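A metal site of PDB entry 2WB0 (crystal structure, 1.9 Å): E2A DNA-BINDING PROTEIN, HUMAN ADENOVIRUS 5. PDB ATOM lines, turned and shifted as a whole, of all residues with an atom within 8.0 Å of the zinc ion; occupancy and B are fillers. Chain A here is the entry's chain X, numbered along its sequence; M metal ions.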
ATOM      1  N   ARG A 222     -16.021 -14.009  -7.442  1.00  0.00           N
ATOM      2  CA  ARG A 222     -17.296 -14.603  -7.858  1.00  0.00           C
ATOM      3  C   ARG A 222     -17.147 -15.522  -9.018  1.00  0.00           C
ATOM      4  O   ARG A 222     -16.448 -15.215  -9.990  1.00  0.00           O
ATOM      5  CB  ARG A 222     -18.281 -13.492  -8.303  1.00  0.00           C
ATOM      6  CG  ARG A 222     -18.354 -12.353  -7.260  1.00  0.00           C
ATOM      7  CD  ARG A 222     -19.488 -11.345  -7.549  1.00  0.00           C
ATOM      8  NE  ARG A 222     -19.472 -10.656  -8.843  1.00  0.00           N
ATOM      9  CZ  ARG A 222     -19.364  -9.336  -9.007  1.00  0.00           C
ATOM     10  NH1 ARG A 222     -19.065  -8.505  -7.975  1.00  0.00           N
ATOM     11  NH2 ARG A 222     -19.437  -8.859 -10.266  1.00  0.00           N
ATOM     12  N   CYS A 223     -17.771 -16.677  -8.907  1.00  0.00           N
ATOM     13  CA  CYS A 223     -17.887 -17.576 -10.038  1.00  0.00           C
ATOM     14  C   CYS A 223     -19.354 -17.377 -10.518  1.00  0.00           C
ATOM     15  O   CYS A 223     -19.942 -16.359 -10.233  1.00  0.00           O
ATOM     16  CB  CYS A 223     -17.557 -19.016  -9.661  1.00  0.00           C
ATOM     17  SG  CYS A 223     -18.715 -19.700  -8.424  1.00  0.00           S
ATOM     18  N   GLU A 224     -19.933 -18.306 -11.273  1.00  0.00           N
ATOM     19  CA  GLU A 224     -21.332 -18.160 -11.714  1.00  0.00           C
ATOM     20  C   GLU A 224     -22.265 -18.281 -10.543  1.00  0.00           C
ATOM     21  O   GLU A 224     -23.285 -17.575 -10.490  1.00  0.00           O
ATOM     22  CB  GLU A 224     -21.669 -19.287 -12.685  1.00  0.00           C
ATOM     23  CG  GLU A 224     -20.808 -19.195 -13.923  1.00  0.00           C
ATOM     24  CD  GLU A 224     -21.119 -20.280 -15.016  1.00  0.00           C
ATOM     25  OE1 GLU A 224     -22.294 -20.764 -15.083  1.00  0.00           O
ATOM     26  OE2 GLU A 224     -20.144 -20.644 -15.762  1.00  0.00           O
ATOM     27  N   CYS A 225     -21.891 -19.133  -9.573  1.00  0.00           N
ATOM     28  CA  CYS A 225     -22.774 -19.420  -8.446  1.00  0.00           C
ATOM     29  C   CYS A 225     -23.115 -18.201  -7.593  1.00  0.00           C
ATOM     30  O   CYS A 225     -24.241 -18.139  -7.083  1.00  0.00           O
ATOM     31  CB  CYS A 225     -22.206 -20.550  -7.545  1.00  0.00           C
ATOM     32  SG  CYS A 225     -21.707 -22.045  -8.490  1.00  0.00           S
ATOM     33  N   ASN A 226     -22.159 -17.302  -7.338  1.00  0.00           N
ATOM     34  CA  ASN A 226     -22.458 -16.092  -6.597  1.00  0.00           C
ATOM     35  C   ASN A 226     -22.215 -14.843  -7.422  1.00  0.00           C
ATOM     36  O   ASN A 226     -21.769 -13.824  -6.873  1.00  0.00           O
ATOM     37  CB  ASN A 226     -21.640 -16.025  -5.285  1.00  0.00           C
ATOM     38  CG  ASN A 226     -20.124 -16.152  -5.529  1.00  0.00           C
ATOM     39  OD1 ASN A 226     -19.665 -16.486  -6.607  1.00  0.00           O
ATOM     40  ND2 ASN A 226     -19.372 -15.933  -4.477  1.00  0.00           N
ATOM     41  N   SER A 227     -22.454 -14.918  -8.712  1.00  0.00           N
ATOM     42  CA  SER A 227     -22.216 -13.699  -9.525  1.00  0.00           C
ATOM     43  C   SER A 227     -23.233 -12.598  -9.169  1.00  0.00           C
ATOM     44  O   SER A 227     -22.906 -11.403  -9.307  1.00  0.00           O
ATOM     45  CB  SER A 227     -22.186 -13.935 -11.046  1.00  0.00           C
ATOM     46  OG  SER A 227     -23.407 -14.538 -11.377  1.00  0.00           O
ATOM     47  N   PHE A 234     -25.433 -20.554  -0.348  1.00  0.00           N
ATOM     48  CA  PHE A 234     -24.994 -21.937  -0.512  1.00  0.00           C
ATOM     49  C   PHE A 234     -23.899 -22.246   0.492  1.00  0.00           C
ATOM     50  O   PHE A 234     -23.262 -21.350   1.056  1.00  0.00           O
ATOM     51  CB  PHE A 234     -24.526 -22.239  -1.952  1.00  0.00           C
ATOM     52  CG  PHE A 234     -23.496 -21.252  -2.488  1.00  0.00           C
ATOM     53  CD1 PHE A 234     -22.129 -21.424  -2.196  1.00  0.00           C
ATOM     54  CD2 PHE A 234     -23.875 -20.213  -3.335  1.00  0.00           C
ATOM     55  CE1 PHE A 234     -21.131 -20.523  -2.685  1.00  0.00           C
ATOM     56  CE2 PHE A 234     -22.881 -19.282  -3.838  1.00  0.00           C
ATOM     57  CZ  PHE A 234     -21.484 -19.485  -3.543  1.00  0.00           C
ATOM     58  N   LEU A 239     -15.800 -18.197  -2.161  1.00  0.00           N
ATOM     59  CA  LEU A 239     -15.141 -17.553  -3.268  1.00  0.00           C
ATOM     60  C   LEU A 239     -14.514 -18.621  -4.123  1.00  0.00           C
ATOM     61  O   LEU A 239     -14.287 -19.730  -3.681  1.00  0.00           O
ATOM     62  CB  LEU A 239     -13.961 -16.610  -2.806  1.00  0.00           C
ATOM     63  CG  LEU A 239     -14.261 -15.660  -1.640  1.00  0.00           C
ATOM     64  CD1 LEU A 239     -13.058 -15.426  -0.680  1.00  0.00           C
ATOM     65  CD2 LEU A 239     -14.731 -14.335  -2.317  1.00  0.00           C
ATOM     66  N   PRO A 240     -14.201 -18.291  -5.378  1.00  0.00           N
ATOM     67  CA  PRO A 240     -13.619 -19.298  -6.276  1.00  0.00           C
ATOM     68  C   PRO A 240     -12.413 -20.056  -5.690  1.00  0.00           C
ATOM     69  O   PRO A 240     -11.484 -19.419  -5.084  1.00  0.00           O
ATOM     70  CB  PRO A 240     -13.175 -18.423  -7.490  1.00  0.00           C
ATOM     71  CG  PRO A 240     -14.407 -17.481  -7.608  1.00  0.00           C
ATOM     72  CD  PRO A 240     -14.651 -17.111  -6.101  1.00  0.00           C
ATOM     73  N   LYS A 241     -12.400 -21.398  -5.822  1.00  0.00           N
ATOM     74  CA  LYS A 241     -11.307 -22.160  -5.277  1.00  0.00           C
ATOM     75  C   LYS A 241      -9.978 -21.764  -5.981  1.00  0.00           C
ATOM     76  O   LYS A 241      -9.959 -21.462  -7.193  1.00  0.00           O
ATOM     77  CB  LYS A 241     -11.508 -23.663  -5.519  1.00  0.00           C
ATOM     78  CG  LYS A 241     -10.576 -24.500  -4.665  1.00  0.00           C
ATOM     79  CD  LYS A 241     -10.880 -26.020  -5.007  1.00  0.00           C
ATOM     80  CE  LYS A 241     -10.173 -27.088  -4.070  1.00  0.00           C
ATOM     81  NZ  LYS A 241      -8.666 -27.002  -4.290  1.00  0.00           N
ATOM     82  N   GLN A 276     -11.275 -21.822  -9.905  1.00  0.00           N
ATOM     83  CA  GLN A 276     -12.433 -22.587 -10.373  1.00  0.00           C
ATOM     84  C   GLN A 276     -13.629 -22.145  -9.596  1.00  0.00           C
ATOM     85  O   GLN A 276     -13.559 -21.141  -8.843  1.00  0.00           O
ATOM     86  CB  GLN A 276     -12.210 -24.141 -10.240  1.00  0.00           C
ATOM     87  CG  GLN A 276     -11.144 -24.593 -11.214  1.00  0.00           C
ATOM     88  CD  GLN A 276     -10.573 -25.965 -10.956  1.00  0.00           C
ATOM     89  OE1 GLN A 276     -10.996 -26.959 -11.594  1.00  0.00           O
ATOM     90  NE2 GLN A 276      -9.651 -26.055 -10.032  1.00  0.00           N
ATOM     91  N   CYS A 277     -14.707 -22.920  -9.734  1.00  0.00           N
ATOM     92  CA  CYS A 277     -15.965 -22.657  -8.988  1.00  0.00           C
ATOM     93  C   CYS A 277     -15.687 -22.504  -7.476  1.00  0.00           C
ATOM     94  O   CYS A 277     -14.712 -23.070  -6.989  1.00  0.00           O
ATOM     95  CB  CYS A 277     -16.895 -23.864  -9.125  1.00  0.00           C
ATOM     96  SG  CYS A 277     -18.491 -23.634  -8.309  1.00  0.00           S
ATOM     97  N   CYS A 278     -16.498 -21.730  -6.742  1.00  0.00           N
ATOM     98  CA  CYS A 278     -16.414 -21.785  -5.254  1.00  0.00           C
ATOM     99  C   CYS A 278     -16.337 -23.241  -4.745  1.00  0.00           C
ATOM    100  O   CYS A 278     -15.536 -23.545  -3.840  1.00  0.00           O
ATOM    101  CB  CYS A 278     -17.625 -21.147  -4.583  1.00  0.00           C
ATOM    102  SG  CYS A 278     -17.701 -19.358  -4.849  1.00  0.00           S
ATOM    103  N   ASN A 279     -17.162 -24.115  -5.317  1.00  0.00           N
ATOM    104  CA  ASN A 279     -17.231 -25.513  -4.866  1.00  0.00           C
ATOM    105  C   ASN A 279     -17.266 -26.441  -6.049  1.00  0.00           C
ATOM    106  O   ASN A 279     -18.311 -26.988  -6.416  1.00  0.00           O
ATOM    107  CB  ASN A 279     -18.449 -25.719  -4.007  1.00  0.00           C
ATOM    108  CG  ASN A 279     -18.488 -24.768  -2.852  1.00  0.00           C
ATOM    109  OD1 ASN A 279     -19.144 -23.701  -2.894  1.00  0.00           O
ATOM    110  ND2 ASN A 279     -17.752 -25.110  -1.807  1.00  0.00           N
ATOM    111  N   PRO A 280     -16.109 -26.669  -6.632  1.00  0.00           N
ATOM    112  CA  PRO A 280     -16.112 -27.509  -7.832  1.00  0.00           C
ATOM    113  C   PRO A 280     -16.438 -28.954  -7.472  1.00  0.00           C
ATOM    114  O   PRO A 280     -16.132 -29.405  -6.375  1.00  0.00           O
ATOM    115  CB  PRO A 280     -14.688 -27.384  -8.395  1.00  0.00           C
ATOM    116  CG  PRO A 280     -13.961 -26.319  -7.532  1.00  0.00           C
ATOM    117  CD  PRO A 280     -14.784 -26.140  -6.246  1.00  0.00           C
ATOM    118  N   PRO A 292     -25.067 -25.490  -5.652  1.00  0.00           N
ATOM    119  CA  PRO A 292     -24.694 -25.090  -7.029  1.00  0.00           C
ATOM    120  C   PRO A 292     -23.219 -25.406  -7.306  1.00  0.00           C
ATOM    121  O   PRO A 292     -22.406 -25.477  -6.370  1.00  0.00           O
ATOM    122  CB  PRO A 292     -24.876 -23.580  -6.993  1.00  0.00           C
ATOM    123  CG  PRO A 292     -24.484 -23.204  -5.498  1.00  0.00           C
ATOM    124  CD  PRO A 292     -25.055 -24.341  -4.695  1.00  0.00           C
ATOM    125  N   ASN A 293     -22.871 -25.621  -8.583  1.00  0.00           N
ATOM    126  CA  ASN A 293     -21.479 -25.688  -9.004  1.00  0.00           C
ATOM    127  C   ASN A 293     -21.448 -25.237 -10.458  1.00  0.00           C
ATOM    128  O   ASN A 293     -22.463 -25.299 -11.126  1.00  0.00           O
ATOM    129  CB  ASN A 293     -20.840 -27.060  -8.871  1.00  0.00           C
ATOM    130  CG  ASN A 293     -21.417 -28.070  -9.843  1.00  0.00           C
ATOM    131  OD1 ASN A 293     -22.396 -28.751  -9.545  1.00  0.00           O
ATOM    132  ND2 ASN A 293     -20.798 -28.199 -11.005  1.00  0.00           N
ATOM    133  N   CYS A 294     -20.331 -24.664 -10.910  1.00  0.00           N
ATOM    134  CA  CYS A 294     -20.326 -24.157 -12.260  1.00  0.00           C
ATOM    135  C   CYS A 294     -18.999 -24.521 -12.919  1.00  0.00           C
ATOM    136  O   CYS A 294     -18.115 -25.010 -12.204  1.00  0.00           O
ATOM    137  CB  CYS A 294     -20.599 -22.702 -12.243  1.00  0.00           C
ATOM    138  SG  CYS A 294     -19.196 -21.741 -11.518  1.00  0.00           S
ATOM    139  N   ASP A 295     -18.827 -24.233 -14.201  1.00  0.00           N
ATOM    140  CA  ASP A 295     -17.620 -24.622 -14.914  1.00  0.00           C
ATOM    141  C   ASP A 295     -16.592 -23.432 -14.985  1.00  0.00           C
ATOM    142  O   ASP A 295     -15.648 -23.446 -15.800  1.00  0.00           O
ATOM    143  CB  ASP A 295     -18.006 -25.104 -16.324  1.00  0.00           C
ATOM    144  CG  ASP A 295     -18.739 -24.011 -17.187  1.00  0.00           C
ATOM    145  OD1 ASP A 295     -18.722 -22.771 -16.834  1.00  0.00           O
ATOM    146  OD2 ASP A 295     -19.343 -24.351 -18.251  1.00  0.00           O
ATOM    147  N   PHE A 296     -16.743 -22.407 -14.122  1.00  0.00           N
ATOM    148  CA  PHE A 296     -15.777 -21.310 -14.125  1.00  0.00           C
ATOM    149  C   PHE A 296     -14.333 -21.847 -14.033  1.00  0.00           C
ATOM    150  O   PHE A 296     -14.023 -22.669 -13.143  1.00  0.00           O
ATOM    151  CB  PHE A 296     -16.132 -20.405 -12.933  1.00  0.00           C
ATOM    152  CG  PHE A 296     -15.289 -19.133 -12.811  1.00  0.00           C
ATOM    153  CD1 PHE A 296     -15.757 -17.910 -13.309  1.00  0.00           C
ATOM    154  CD2 PHE A 296     -14.091 -19.152 -12.101  1.00  0.00           C
ATOM    155  CE1 PHE A 296     -14.967 -16.714 -13.169  1.00  0.00           C
ATOM    156  CE2 PHE A 296     -13.270 -17.935 -11.899  1.00  0.00           C
ATOM    157  CZ  PHE A 296     -13.691 -16.738 -12.440  1.00  0.00           C
HETATM  158 ZN    ZN M   1     -19.486 -21.802  -9.228  1.00  0.00          ZN
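OD1 of Asn 226 sits at hydrogen-bond distance from N of Cys 223 (3.0 Å).
The backbone NH (N) of Glu 224 lies close to the side-chain sulfur (SG) of Cys 294, at 3.5 Å.
The side-chain sulfur (SG) of Cys 225 lies close to the backbone NH (N) of Asn 293 (3.8 Å).
The backbone carbonyl oxygen (O) of Phe 296 sits at hydrogen-bond distance from the backbone NH (N) of Cys 277 (3.5 Å).
SG of Cys 277 lies close to N of Asn 279, 3.3 Å away.
The backbone carbonyl oxygen of Cys 277 lies within hydrogen-bond range of the backbone NH of Lys 241.
SG of Cys 294 sits close to N of Phe 296 (3.6 Å).
The side-chain sulfur (SG) of Cys 278 lies close to the backbone NH (N) of Leu 239 (3.5 Å).
Merely in contact with the zinc ion: Cys 278 (3.9 Å).
Within 4 Å of the zinc ion: Cys 223, Cys 225, Cys 277, Cys 278 and Cys 294.
The zinc ion is bound by the side-chain sulfur of Cys 277, the side-chain sulfur of Cys 294, the side-chain sulfur of Cys 225 and the side-chain sulfur of Cys 223.
The zinc ion has four donor atoms within binding distance.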
